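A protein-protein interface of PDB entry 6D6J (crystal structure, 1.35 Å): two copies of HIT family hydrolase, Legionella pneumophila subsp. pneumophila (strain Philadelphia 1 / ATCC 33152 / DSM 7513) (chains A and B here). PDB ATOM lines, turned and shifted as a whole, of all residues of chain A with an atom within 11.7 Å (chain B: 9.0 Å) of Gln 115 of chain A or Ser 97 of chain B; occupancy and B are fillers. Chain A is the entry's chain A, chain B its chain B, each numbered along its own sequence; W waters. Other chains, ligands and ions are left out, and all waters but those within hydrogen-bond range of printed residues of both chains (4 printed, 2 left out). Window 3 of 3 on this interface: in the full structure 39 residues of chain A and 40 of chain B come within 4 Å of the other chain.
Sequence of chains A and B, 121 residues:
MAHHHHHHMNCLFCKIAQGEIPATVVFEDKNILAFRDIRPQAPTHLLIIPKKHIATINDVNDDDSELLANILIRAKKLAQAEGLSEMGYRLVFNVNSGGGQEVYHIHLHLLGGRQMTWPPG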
ATOM      1  N   GLN A  41       5.100   0.324 -16.127  1.00  0.00           N
ATOM      2  CA  GLN A  41       4.858   1.277 -17.203  1.00  0.00           C
ATOM      3  C   GLN A  41       5.550   0.872 -18.487  1.00  0.00           C
ATOM      4  O   GLN A  41       5.503   1.616 -19.472  1.00  0.00           O
ATOM      5  CB  GLN A  41       5.298   2.680 -16.784  1.00  0.00           C
ATOM      6  CG  GLN A  41       4.614   3.186 -15.522  1.00  0.00           C
ATOM      7  CD  GLN A  41       3.112   3.304 -15.692  1.00  0.00           C
ATOM      8  OE1 GLN A  41       2.623   4.150 -16.438  1.00  0.00           O
ATOM      9  NE2 GLN A  41       2.373   2.432 -15.021  1.00  0.00           N
ATOM     10  N   ALA A  42       6.209  -0.279 -18.476  1.00  0.00           N
ATOM     11  CA  ALA A  42       6.883  -0.842 -19.634  1.00  0.00           C
ATOM     12  C   ALA A  42       6.991  -2.331 -19.392  1.00  0.00           C
ATOM     13  O   ALA A  42       6.828  -2.780 -18.253  1.00  0.00           O
ATOM     14  CB  ALA A  42       8.286  -0.225 -19.804  1.00  0.00           C
ATOM     15  N   PRO A  43       7.237  -3.130 -20.433  1.00  0.00           N
ATOM     16  CA  PRO A  43       7.339  -4.578 -20.203  1.00  0.00           C
ATOM     17  C   PRO A  43       8.364  -4.936 -19.141  1.00  0.00           C
ATOM     18  O   PRO A  43       8.125  -5.840 -18.335  1.00  0.00           O
ATOM     19  CB  PRO A  43       7.665  -5.114 -21.597  1.00  0.00           C
ATOM     20  CG  PRO A  43       6.962  -4.134 -22.509  1.00  0.00           C
ATOM     21  CD  PRO A  43       7.224  -2.801 -21.869  1.00  0.00           C
ATOM     22  N   THR A  44       9.499  -4.247 -19.104  1.00  0.00           N
ATOM     23  CA  THR A  44      10.405  -4.291 -17.961  1.00  0.00           C
ATOM     24  C   THR A  44      10.229  -3.008 -17.170  1.00  0.00           C
ATOM     25  O   THR A  44      10.424  -1.914 -17.702  1.00  0.00           O
ATOM     26  CB  THR A  44      11.866  -4.385 -18.405  1.00  0.00           C
ATOM     27  OG1 THR A  44      12.079  -5.605 -19.112  1.00  0.00           O
ATOM     28  CG2 THR A  44      12.788  -4.319 -17.184  1.00  0.00           C
ATOM     29  N   GLY A  83      17.925  -8.382 -21.087  1.00  0.00           N
ATOM     30  CA  GLY A  83      17.944  -8.343 -22.540  1.00  0.00           C
ATOM     31  C   GLY A  83      17.823  -6.960 -23.140  1.00  0.00           C
ATOM     32  O   GLY A  83      17.523  -6.833 -24.336  1.00  0.00           O
ATOM     33  N   LEU A  84      18.045  -5.913 -22.352  1.00  0.00           N
ATOM     34  CA  LEU A  84      17.766  -4.545 -22.778  1.00  0.00           C
ATOM     35  C   LEU A  84      18.994  -3.744 -23.175  1.00  0.00           C
ATOM     36  O   LEU A  84      18.836  -2.599 -23.605  1.00  0.00           O
ATOM     37  CB  LEU A  84      17.079  -3.782 -21.648  1.00  0.00           C
ATOM     38  CG  LEU A  84      15.803  -4.423 -21.135  1.00  0.00           C
ATOM     39  CD1 LEU A  84      15.262  -3.573 -19.999  1.00  0.00           C
ATOM     40  CD2 LEU A  84      14.779  -4.572 -22.273  1.00  0.00           C
ATOM     41  N   SER A  85      20.208  -4.282 -23.047  1.00  0.00           N
ATOM     42  CA  SER A  85      21.400  -3.448 -23.218  1.00  0.00           C
ATOM     43  C   SER A  85      21.398  -2.729 -24.558  1.00  0.00           C
ATOM     44  O   SER A  85      21.673  -1.520 -24.635  1.00  0.00           O
ATOM     45  CB  SER A  85      22.667  -4.294 -23.106  1.00  0.00           C
ATOM     46  OG  SER A  85      22.842  -4.809 -21.806  1.00  0.00           O
ATOM     47  N   GLU A  86      21.120  -3.468 -25.638  1.00  0.00           N
ATOM     48  CA  GLU A  86      21.144  -2.889 -26.976  1.00  0.00           C
ATOM     49  C   GLU A  86      19.785  -2.372 -27.418  1.00  0.00           C
ATOM     50  O   GLU A  86      19.711  -1.315 -28.050  1.00  0.00           O
ATOM     51  CB  GLU A  86      21.697  -3.899 -27.984  1.00  0.00           C
ATOM     52  CG  GLU A  86      23.165  -4.194 -27.755  1.00  0.00           C
ATOM     53  CD  GLU A  86      24.010  -2.923 -27.769  1.00  0.00           C
ATOM     54  OE1 GLU A  86      23.900  -2.138 -28.740  1.00  0.00           O
ATOM     55  OE2 GLU A  86      24.746  -2.678 -26.792  1.00  0.00           O
ATOM     56  N   MET A  87      18.710  -3.083 -27.077  1.00  0.00           N
ATOM     57  CA  MET A  87      17.357  -2.624 -27.377  1.00  0.00           C
ATOM     58  C   MET A  87      17.119  -1.233 -26.797  1.00  0.00           C
ATOM     59  O   MET A  87      16.444  -0.400 -27.407  1.00  0.00           O
ATOM     60  CB  MET A  87      16.364  -3.636 -26.783  1.00  0.00           C
ATOM     61  CG  MET A  87      14.889  -3.439 -27.131  1.00  0.00           C
ATOM     62  SD  MET A  87      13.782  -4.470 -26.111  1.00  0.00           S
ATOM     63  CE  MET A  87      14.256  -6.104 -26.670  1.00  0.00           C
ATOM     64  N   GLY A  88      17.661  -0.974 -25.613  1.00  0.00           N
ATOM     65  CA  GLY A  88      17.612   0.317 -24.964  1.00  0.00           C
ATOM     66  C   GLY A  88      16.778   0.293 -23.693  1.00  0.00           C
ATOM     67  O   GLY A  88      15.915  -0.562 -23.488  1.00  0.00           O
ATOM     68  N   TYR A  89      17.044   1.261 -22.824  1.00  0.00           N
ATOM     69  CA  TYR A  89      16.326   1.344 -21.559  1.00  0.00           C
ATOM     70  C   TYR A  89      16.495   2.754 -21.009  1.00  0.00           C
ATOM     71  O   TYR A  89      17.298   3.556 -21.509  1.00  0.00           O
ATOM     72  CB  TYR A  89      16.787   0.282 -20.550  1.00  0.00           C
ATOM     73  CG  TYR A  89      18.258   0.311 -20.204  1.00  0.00           C
ATOM     74  CD1 TYR A  89      19.207  -0.296 -21.025  1.00  0.00           C
ATOM     75  CD2 TYR A  89      18.707   0.933 -19.034  1.00  0.00           C
ATOM     76  CE1 TYR A  89      20.561  -0.271 -20.683  1.00  0.00           C
ATOM     77  CE2 TYR A  89      20.047   0.957 -18.689  1.00  0.00           C
ATOM     78  CZ  TYR A  89      20.972   0.356 -19.518  1.00  0.00           C
ATOM     79  OH  TYR A  89      22.305   0.392 -19.156  1.00  0.00           O
ATOM     80  N   ARG A  90      15.708   3.056 -19.982  1.00  0.00           N
ATOM     81  CA  ARG A  90      15.700   4.374 -19.362  1.00  0.00           C
ATOM     82  C   ARG A  90      15.781   4.211 -17.851  1.00  0.00           C
ATOM     83  O   ARG A  90      15.123   3.332 -17.283  1.00  0.00           O
ATOM     84  CB  ARG A  90      14.410   5.128 -19.752  1.00  0.00           C
ATOM     85  CG  ARG A  90      14.259   6.470 -19.063  1.00  0.00           C
ATOM     86  CD  ARG A  90      13.149   7.307 -19.691  1.00  0.00           C
ATOM     87  NE  ARG A  90      13.559   7.694 -21.036  1.00  0.00           N
ATOM     88  CZ  ARG A  90      12.744   8.157 -21.982  1.00  0.00           C
ATOM     89  NH1 ARG A  90      11.427   8.325 -21.759  1.00  0.00           N
ATOM     90  NH2 ARG A  90      13.259   8.465 -23.168  1.00  0.00           N
ATOM     91  N   LEU A  91      16.609   5.044 -17.211  1.00  0.00           N
ATOM     92  CA  LEU A  91      16.754   5.089 -15.760  1.00  0.00           C
ATOM     93  C   LEU A  91      16.173   6.402 -15.264  1.00  0.00           C
ATOM     94  O   LEU A  91      16.500   7.457 -15.815  1.00  0.00           O
ATOM     95  CB  LEU A  91      18.236   5.009 -15.379  1.00  0.00           C
ATOM     96  CG  LEU A  91      18.984   3.793 -15.917  1.00  0.00           C
ATOM     97  CD1 LEU A  91      20.438   3.827 -15.492  1.00  0.00           C
ATOM     98  CD2 LEU A  91      18.318   2.488 -15.463  1.00  0.00           C
ATOM     99  N   VAL A  92      15.318   6.343 -14.231  1.00  0.00           N
ATOM    100  CA  VAL A  92      14.624   7.538 -13.740  1.00  0.00           C
ATOM    101  C   VAL A  92      14.691   7.617 -12.218  1.00  0.00           C
ATOM    102  O   VAL A  92      14.330   6.653 -11.529  1.00  0.00           O
ATOM    103  CB  VAL A  92      13.150   7.565 -14.180  1.00  0.00           C
ATOM    104  CG1 VAL A  92      12.455   8.842 -13.704  1.00  0.00           C
ATOM    105  CG2 VAL A  92      13.009   7.418 -15.680  1.00  0.00           C
ATOM    106  N   LEU A 110      13.994   1.398 -13.595  1.00  0.00           N
ATOM    107  CA  LEU A 110      14.602   0.882 -14.818  1.00  0.00           C
ATOM    108  C   LEU A 110      13.460   0.441 -15.722  1.00  0.00           C
ATOM    109  O   LEU A 110      12.694  -0.467 -15.366  1.00  0.00           O
ATOM    110  CB  LEU A 110      15.557  -0.280 -14.508  1.00  0.00           C
ATOM    111  CG  LEU A 110      15.949  -1.232 -15.660  1.00  0.00           C
ATOM    112  CD1 LEU A 110      16.627  -0.507 -16.807  1.00  0.00           C
ATOM    113  CD2 LEU A 110      16.835  -2.383 -15.176  1.00  0.00           C
ATOM    114  N   LEU A 111      13.339   1.085 -16.878  1.00  0.00           N
ATOM    115  CA  LEU A 111      12.234   0.837 -17.801  1.00  0.00           C
ATOM    116  C   LEU A 111      12.764   0.444 -19.167  1.00  0.00           C
ATOM    117  O   LEU A 111      13.701   1.059 -19.670  1.00  0.00           O
ATOM    118  CB  LEU A 111      11.393   2.110 -17.962  1.00  0.00           C
ATOM    119  CG  LEU A 111      10.704   2.576 -16.685  1.00  0.00           C
ATOM    120  CD1 LEU A 111      10.880   4.068 -16.517  1.00  0.00           C
ATOM    121  CD2 LEU A 111       9.254   2.183 -16.778  1.00  0.00           C
ATOM    122  N   GLY A 112      12.141  -0.553 -19.783  1.00  0.00           N
ATOM    123  CA  GLY A 112      12.495  -0.892 -21.148  1.00  0.00           C
ATOM    124  C   GLY A 112      11.582  -1.969 -21.686  1.00  0.00           C
ATOM    125  O   GLY A 112      10.592  -2.351 -21.053  1.00  0.00           O
ATOM    126  N   GLY A 113      11.937  -2.480 -22.860  1.00  0.00           N
ATOM    127  CA  GLY A 113      11.131  -3.478 -23.526  1.00  0.00           C
ATOM    128  C   GLY A 113      10.105  -2.893 -24.458  1.00  0.00           C
ATOM    129  O   GLY A 113       9.318  -3.647 -25.038  1.00  0.00           O
ATOM    130  N   ARG A 114      10.078  -1.573 -24.601  1.00  0.00           N
ATOM    131  CA  ARG A 114       9.302  -0.849 -25.600  1.00  0.00           C
ATOM    132  C   ARG A 114      10.105   0.405 -25.903  1.00  0.00           C
ATOM    133  O   ARG A 114      11.055   0.742 -25.182  1.00  0.00           O
ATOM    134  CB  ARG A 114       7.925  -0.426 -25.073  1.00  0.00           C
ATOM    135  CG  ARG A 114       7.973   0.524 -23.867  1.00  0.00           C
ATOM    136  CD  ARG A 114       6.619   1.143 -23.615  1.00  0.00           C
ATOM    137  NE  ARG A 114       6.494   1.877 -22.360  1.00  0.00           N
ATOM    138  CZ  ARG A 114       6.780   3.169 -22.212  1.00  0.00           C
ATOM    139  NH1 ARG A 114       7.265   3.888 -23.222  1.00  0.00           N
ATOM    140  NH2 ARG A 114       6.584   3.737 -21.038  1.00  0.00           N
ATOM    141  N   GLN A 115       9.724   1.111 -26.963  1.00  0.00           N
ATOM    142  CA  GLN A 115      10.326   2.409 -27.228  1.00  0.00           C
ATOM    143  C   GLN A 115       9.963   3.379 -26.110  1.00  0.00           C
ATOM    144  O   GLN A 115       8.780   3.577 -25.803  1.00  0.00           O
ATOM    145  CB  GLN A 115       9.812   2.965 -28.554  1.00  0.00           C
ATOM    146  CG  GLN A 115      10.420   4.334 -28.907  1.00  0.00           C
ATOM    147  CD  GLN A 115      11.916   4.269 -29.117  1.00  0.00           C
ATOM    148  OE1 GLN A 115      12.410   3.483 -29.921  1.00  0.00           O
ATOM    149  NE2 GLN A 115      12.651   5.094 -28.386  1.00  0.00           N
ATOM    150  N   MET A 116      10.976   3.992 -25.499  1.00  0.00           N
ATOM    151  CA  MET A 116      10.756   5.052 -24.522  1.00  0.00           C
ATOM    152  C   MET A 116      10.696   6.384 -25.261  1.00  0.00           C
ATOM    153  O   MET A 116      11.467   6.614 -26.194  1.00  0.00           O
ATOM    154  CB  MET A 116      11.891   5.051 -23.496  1.00  0.00           C
ATOM    155  CG  MET A 116      12.095   3.694 -22.795  1.00  0.00           C
ATOM    156  SD  MET A 116      10.607   3.000 -22.006  1.00  0.00           S
ATOM    157  CE  MET A 116      10.235   4.299 -20.805  1.00  0.00           C
ATOM    158  N   THR A 117       9.757   7.236 -24.871  1.00  0.00           N
ATOM    159  CA  THR A 117       9.397   8.404 -25.670  1.00  0.00           C
ATOM    160  C   THR A 117       9.797   9.705 -24.975  1.00  0.00           C
ATOM    161  O   THR A 117      10.196   9.730 -23.812  1.00  0.00           O
ATOM    162  CB  THR A 117       7.902   8.390 -26.043  1.00  0.00           C
ATOM    163  OG1 THR A 117       7.095   8.568 -24.875  1.00  0.00           O
ATOM    164  CG2 THR A 117       7.532   7.065 -26.713  1.00  0.00           C
ATOM    165  N   TRP A 118       9.670  10.804 -25.712  1.00  0.00           N
ATOM    166  CA  TRP A 118      10.137  12.110 -25.277  1.00  0.00           C
ATOM    167  C   TRP A 118       8.976  13.077 -25.478  1.00  0.00           C
ATOM    168  O   TRP A 118       8.384  13.090 -26.563  1.00  0.00           O
ATOM    169  CB  TRP A 118      11.330  12.537 -26.140  1.00  0.00           C
ATOM    170  CG  TRP A 118      12.359  13.400 -25.440  1.00  0.00           C
ATOM    171  CD1 TRP A 118      12.790  14.648 -25.823  1.00  0.00           C
ATOM    172  CD2 TRP A 118      13.085  13.080 -24.245  1.00  0.00           C
ATOM    173  NE1 TRP A 118      13.749  15.100 -24.956  1.00  0.00           N
ATOM    174  CE2 TRP A 118      13.949  14.160 -23.977  1.00  0.00           C
ATOM    175  CE3 TRP A 118      13.102  11.975 -23.384  1.00  0.00           C
ATOM    176  CZ2 TRP A 118      14.809  14.179 -22.872  1.00  0.00           C
ATOM    177  CZ3 TRP A 118      13.972  11.984 -22.293  1.00  0.00           C
ATOM    178  CH2 TRP A 118      14.810  13.091 -22.046  1.00  0.00           C
ATOM    179  N   PRO A 119       8.614  13.908 -24.485  1.00  0.00           N
ATOM    180  CA  PRO A 119       9.292  14.127 -23.200  1.00  0.00           C
ATOM    181  C   PRO A 119       9.114  12.959 -22.214  1.00  0.00           C
ATOM    182  O   PRO A 119       8.179  12.160 -22.322  1.00  0.00           O
ATOM    183  CB  PRO A 119       8.581  15.371 -22.658  1.00  0.00           C
ATOM    184  CG  PRO A 119       7.183  15.259 -23.223  1.00  0.00           C
ATOM    185  CD  PRO A 119       7.430  14.783 -24.637  1.00  0.00           C
ATOM    186  N   PRO A 120       9.977  12.890 -21.210  1.00  0.00           N
ATOM    187  CA  PRO A 120       9.893  11.802 -20.224  1.00  0.00           C
ATOM    188  C   PRO A 120       8.935  12.173 -19.096  1.00  0.00           C
ATOM    189  O   PRO A 120       9.324  12.331 -17.923  1.00  0.00           O
ATOM    190  CB  PRO A 120      11.342  11.705 -19.743  1.00  0.00           C
ATOM    191  CG  PRO A 120      11.784  13.164 -19.716  1.00  0.00           C
ATOM    192  CD  PRO A 120      11.136  13.775 -20.956  1.00  0.00           C
ATOM    193  N   GLY A 121       7.655  12.314 -19.450  1.00  0.00           N
ATOM    194  CA  GLY A 121       6.652  12.846 -18.542  1.00  0.00           C
ATOM    195  C   GLY A 121       6.794  14.336 -18.345  1.00  0.00           C
ATOM    196  O   GLY A 121       7.276  15.015 -19.260  1.00  0.00           O
ATOM    197  OXT GLY A 121       6.423  14.867 -17.285  1.00  0.00           O
ATOM    198  N   THR B  56      27.724   5.305 -23.728  1.00  0.00           N
ATOM    199  CA  THR B  56      26.449   4.953 -23.104  1.00  0.00           C
ATOM    200  C   THR B  56      26.689   4.463 -21.683  1.00  0.00           C
ATOM    201  O   THR B  56      27.815   4.135 -21.296  1.00  0.00           O
ATOM    202  CB  THR B  56      25.692   3.836 -23.851  1.00  0.00           C
ATOM    203  OG1 THR B  56      26.306   2.574 -23.568  1.00  0.00           O
ATOM    204  CG2 THR B  56      25.632   4.077 -25.359  1.00  0.00           C
ATOM    205  N   ASN B  58      26.037   1.632 -20.702  1.00  0.00           N
ATOM    206  CA  ASN B  58      26.576   0.275 -20.788  1.00  0.00           C
ATOM    207  C   ASN B  58      28.096   0.256 -20.801  1.00  0.00           C
ATOM    208  O   ASN B  58      28.691  -0.789 -20.519  1.00  0.00           O
ATOM    209  CB  ASN B  58      26.086  -0.438 -22.049  1.00  0.00           C
ATOM    210  CG  ASN B  58      24.593  -0.604 -22.085  1.00  0.00           C
ATOM    211  OD1 ASN B  58      23.946  -0.767 -21.055  1.00  0.00           O
ATOM    212  ND2 ASN B  58      24.026  -0.547 -23.277  1.00  0.00           N
ATOM    213  N   ASN B  94      19.006   8.142 -20.511  1.00  0.00           N
ATOM    214  CA  ASN B  94      18.538   7.352 -21.642  1.00  0.00           C
ATOM    215  C   ASN B  94      19.685   6.486 -22.132  1.00  0.00           C
ATOM    216  O   ASN B  94      20.830   6.942 -22.181  1.00  0.00           O
ATOM    217  CB  ASN B  94      18.114   8.275 -22.779  1.00  0.00           C
ATOM    218  CG  ASN B  94      16.851   9.045 -22.459  1.00  0.00           C
ATOM    219  OD1 ASN B  94      16.116   8.709 -21.530  1.00  0.00           O
ATOM    220  ND2 ASN B  94      16.564  10.059 -23.265  1.00  0.00           N
ATOM    221  N   VAL B  95      19.384   5.248 -22.522  1.00  0.00           N
ATOM    222  CA  VAL B  95      20.422   4.333 -22.990  1.00  0.00           C
ATOM    223  C   VAL B  95      20.001   3.736 -24.325  1.00  0.00           C
ATOM    224  O   VAL B  95      19.032   2.961 -24.395  1.00  0.00           O
ATOM    225  CB  VAL B  95      20.753   3.240 -21.962  1.00  0.00           C
ATOM    226  CG1 VAL B  95      21.989   2.455 -22.417  1.00  0.00           C
ATOM    227  CG2 VAL B  95      20.982   3.864 -20.585  1.00  0.00           C
ATOM    228  N   ASN B  96      20.744   4.077 -25.375  1.00  0.00           N
ATOM    229  CA  ASN B  96      20.541   3.570 -26.729  1.00  0.00           C
ATOM    230  C   ASN B  96      19.230   4.052 -27.346  1.00  0.00           C
ATOM    231  O   ASN B  96      18.449   4.765 -26.706  1.00  0.00           O
ATOM    232  CB  ASN B  96      20.787   2.054 -26.819  1.00  0.00           C
ATOM    233  CG  ASN B  96      22.263   1.743 -26.842  1.00  0.00           C
ATOM    234  OD1 ASN B  96      23.030   2.522 -27.400  1.00  0.00           O
ATOM    235  ND2 ASN B  96      22.676   0.643 -26.220  1.00  0.00           N
ATOM    236  N   SER B  97      18.990   3.701 -28.603  1.00  0.00           N
ATOM    237  CA  SER B  97      17.878   4.309 -29.322  1.00  0.00           C
ATOM    238  C   SER B  97      16.543   3.980 -28.668  1.00  0.00           C
ATOM    239  O   SER B  97      15.665   4.844 -28.577  1.00  0.00           O
ATOM    240  CB  SER B  97      17.892   3.884 -30.794  1.00  0.00           C
ATOM    241  OG  SER B  97      16.904   4.595 -31.524  1.00  0.00           O
ATOM    242  N   GLY B  98      16.359   2.737 -28.211  1.00  0.00           N
ATOM    243  CA  GLY B  98      15.104   2.369 -27.584  1.00  0.00           C
ATOM    244  C   GLY B  98      14.863   3.087 -26.277  1.00  0.00           C
ATOM    245  O   GLY B  98      13.710   3.201 -25.843  1.00  0.00           O
ATOM    246  N   GLY B  99      15.930   3.563 -25.627  1.00  0.00           N
ATOM    247  CA  GLY B  99      15.809   4.387 -24.440  1.00  0.00           C
ATOM    248  C   GLY B  99      15.675   5.861 -24.722  1.00  0.00           C
ATOM    249  O   GLY B  99      15.506   6.636 -23.778  1.00  0.00           O
ATOM    250  N   GLY B 100      15.763   6.278 -25.987  1.00  0.00           N
ATOM    251  CA  GLY B 100      15.665   7.672 -26.363  1.00  0.00           C
ATOM    252  C   GLY B 100      16.989   8.394 -26.524  1.00  0.00           C
ATOM    253  O   GLY B 100      16.990   9.609 -26.748  1.00  0.00           O
ATOM    254  N   GLN B 101      18.115   7.696 -26.399  1.00  0.00           N
ATOM    255  CA  GLN B 101      19.406   8.358 -26.519  1.00  0.00           C
ATOM    256  C   GLN B 101      19.678   8.711 -27.974  1.00  0.00           C
ATOM    257  O   GLN B 101      19.543   7.862 -28.854  1.00  0.00           O
ATOM    258  CB  GLN B 101      20.515   7.438 -25.996  1.00  0.00           C
ATOM    259  CG  GLN B 101      21.883   8.107 -26.036  1.00  0.00           C
ATOM    260  CD  GLN B 101      22.973   7.331 -25.327  1.00  0.00           C
ATOM    261  OE1 GLN B 101      22.796   6.170 -24.939  1.00  0.00           O
ATOM    262  NE2 GLN B 101      24.113   7.980 -25.138  1.00  0.00           N
ATOM    263  N   GLU B 102      20.070   9.953 -28.224  1.00  0.00           N
ATOM    264  CA  GLU B 102      20.446  10.380 -29.572  1.00  0.00           C
ATOM    265  C   GLU B 102      21.902  10.795 -29.685  1.00  0.00           C
ATOM    266  O   GLU B 102      22.530  10.578 -30.733  1.00  0.00           O
ATOM    267  CB  GLU B 102      19.561  11.551 -30.022  1.00  0.00           C
ATOM    268  N   VAL B 103      22.456  11.403 -28.638  1.00  0.00           N
ATOM    269  CA  VAL B 103      23.853  11.812 -28.600  1.00  0.00           C
ATOM    270  C   VAL B 103      24.597  10.763 -27.795  1.00  0.00           C
ATOM    271  O   VAL B 103      24.250  10.493 -26.633  1.00  0.00           O
ATOM    272  CB  VAL B 103      24.018  13.210 -27.980  1.00  0.00           C
ATOM    273  CG1 VAL B 103      25.494  13.570 -27.872  1.00  0.00           C
ATOM    274  CG2 VAL B 103      23.295  14.251 -28.814  1.00  0.00           C
ATOM    275  N   TYR B 104      25.629  10.180 -28.407  1.00  0.00           N
ATOM    276  CA  TYR B 104      26.350   9.045 -27.825  1.00  0.00           C
ATOM    277  C   TYR B 104      27.540   9.505 -26.969  1.00  0.00           C
ATOM    278  O   TYR B 104      28.699   9.153 -27.173  1.00  0.00           O
ATOM    279  CB  TYR B 104      26.673   7.990 -28.894  1.00  0.00           C
ATOM    280  CG  TYR B 104      25.404   7.234 -29.187  1.00  0.00           C
ATOM    281  CD1 TYR B 104      24.475   7.703 -30.107  1.00  0.00           C
ATOM    282  CD2 TYR B 104      25.059   6.126 -28.427  1.00  0.00           C
ATOM    283  CE1 TYR B 104      23.261   7.044 -30.296  1.00  0.00           C
ATOM    284  CE2 TYR B 104      23.882   5.466 -28.609  1.00  0.00           C
ATOM    285  CZ  TYR B 104      22.982   5.914 -29.542  1.00  0.00           C
ATOM    286  OH  TYR B 104      21.798   5.232 -29.691  1.00  0.00           O
ATOM    287  N   PRO B 120       7.067   8.122 -17.366  1.00  0.00           N
ATOM    288  CA  PRO B 120       8.125   9.069 -17.786  1.00  0.00           C
ATOM    289  C   PRO B 120       8.540   8.790 -19.227  1.00  0.00           C
ATOM    290  O   PRO B 120       9.674   8.385 -19.527  1.00  0.00           O
ATOM    291  CB  PRO B 120       9.245   8.753 -16.794  1.00  0.00           C
ATOM    292  CG  PRO B 120       9.118   7.260 -16.610  1.00  0.00           C
ATOM    293  CD  PRO B 120       7.639   6.949 -16.674  1.00  0.00           C
ATOM    294  N   GLY B 121       7.600   9.009 -20.146  1.00  0.00           N
ATOM    295  CA  GLY B 121       7.776   8.591 -21.527  1.00  0.00           C
ATOM    296  C   GLY B 121       7.610   7.098 -21.698  1.00  0.00           C
ATOM    297  O   GLY B 121       8.045   6.516 -22.697  1.00  0.00           O
ATOM    298  OXT GLY B 121       7.043   6.446 -20.812  1.00  0.00           O
HETATM  299  O   HOH W   1      18.252   0.793 -29.326  1.00  0.00           O
HETATM  300  O   HOH W   2      25.468  -0.298 -25.758  1.00  0.00           O
HETATM  301  O   HOH W   3       4.694   5.819 -22.060  1.00  0.00           O
HETATM  302  O   HOH W   4      23.600  -3.180 -19.768  1.00  0.00           O
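O of Ser 85 of chain A sits at hydrogen-bond distance from ND2 of Asn 96 of chain B (2.9 Å).
N of Met 116 of chain A is in hydrogen-bond range of O of Gly 98 of chain B.
The side-chain amide nitrogen (NE2) of Gln 115 of chain A is in hydrogen-bond range of the backbone carbonyl oxygen (O) of Ser 97 of chain B, 3.0 Å away.
The guanidinium group (NE) of Arg 90 of chain A is in hydrogen-bond range of the side-chain amide oxygen (OD1) of Asn 94 of chain B (2.8 Å).
The side-chain amide nitrogen (NE2) of Gln 115 of chain A sits at hydrogen-bond distance from the backbone carbonyl oxygen (O) of Gly 98 of chain B (3.3 Å).
The side-chain amide nitrogen of Asn 58 of chain B sits at hydrogen-bond distance from the backbone carbonyl oxygen of Ser 85 of chain A (2.9 Å).
OXT of Gly 121 of chain B is in salt-bridge range of NH2 of Arg 114 of chain A, 2.8 Å away.
OH of Tyr 89 of chain A is in hydrogen-bond range of OD1 of Asn 58 of chain B (2.8 Å).
NH2 of Arg 90 of chain A lies within hydrogen-bond range of O of Gly 99 of chain B, 3.0 Å away.
The backbone carbonyl oxygen of Met 87 of chain A sits close to the backbone NH of Gly 98 of chain B.
The backbone NH of Gly 121 of chain A sits close to the backbone NH of Gly 121 of chain B (3.4 Å).
The backbone NH of Val 95 of chain B sits at hydrogen-bond distance from the backbone carbonyl oxygen of Tyr 89 of chain A, 2.9 Å away.
NH1 of Arg 90 of chain A sits at hydrogen-bond distance from O of Pro 120 of chain B (2.8 Å).
N of Thr 117 of chain A sits at hydrogen-bond distance from O of Gly 121 of chain B, at 2.9 Å.
The chain-end carboxylate (O) of Gly 121 of chain B is in salt-bridge range of the guanidinium group (NH1) of Arg 90 of chain A (3.9 Å).
N of Arg 90 of chain A sits at hydrogen-bond distance from O of Leu 111 of chain A.
The side-chain amide oxygen (OE1) of Gln 101 of chain B sits at hydrogen-bond distance from the backbone NH (N) of Asn 96 of chain B (3.0 Å).
Of the printed residues of chain A, Ser 97 of chain B touches Gln 115.
Of chain A, only Gly 88, Tyr 89, Arg 90 and Met 116 come within 4 Å of Gly 99 of chain B.
No residue of chain A comes within 4 Å of Gly 100 of chain B.
No residue of chain A comes within 4 Å of Gln 101 of chain B.
Of the printed residues of chain B, Pro 119 of chain A touches Gly 121 (3.7 Å).
Printed residues of chain B within 4 Å of Leu 111 of chain A: Pro 120 (3.6 Å).
The nearest printed residue of chain B that does not touch Gln 115 of chain A is Gly 100 of chain B (4.1 Å).
The nearest printed residue of chain A that does not touch Ser 97 of chain B is Met 87 of chain A (4.6 Å).
Printed residues of chain B that touch a printed residue of chain A: Asn 58, Asn 94, Val 95, Asn 96, Ser 97, Gly 98, Gly 99, Pro 120 and Gly 121.
Of the 26 printed residues of chain A, 15 touch a printed residue of chain B.
Among the printed residues, no Asp or Glu carboxylate lies within 4 Å of a Lys or Arg side-chain nitrogen of the other chain.
Pro 120 of chain B touches its own counterpart, Pro 120 of chain A.
Gly 121 of chain A touches its own counterpart, Gly 121 of chain B.
2 positions are printed for both chains.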
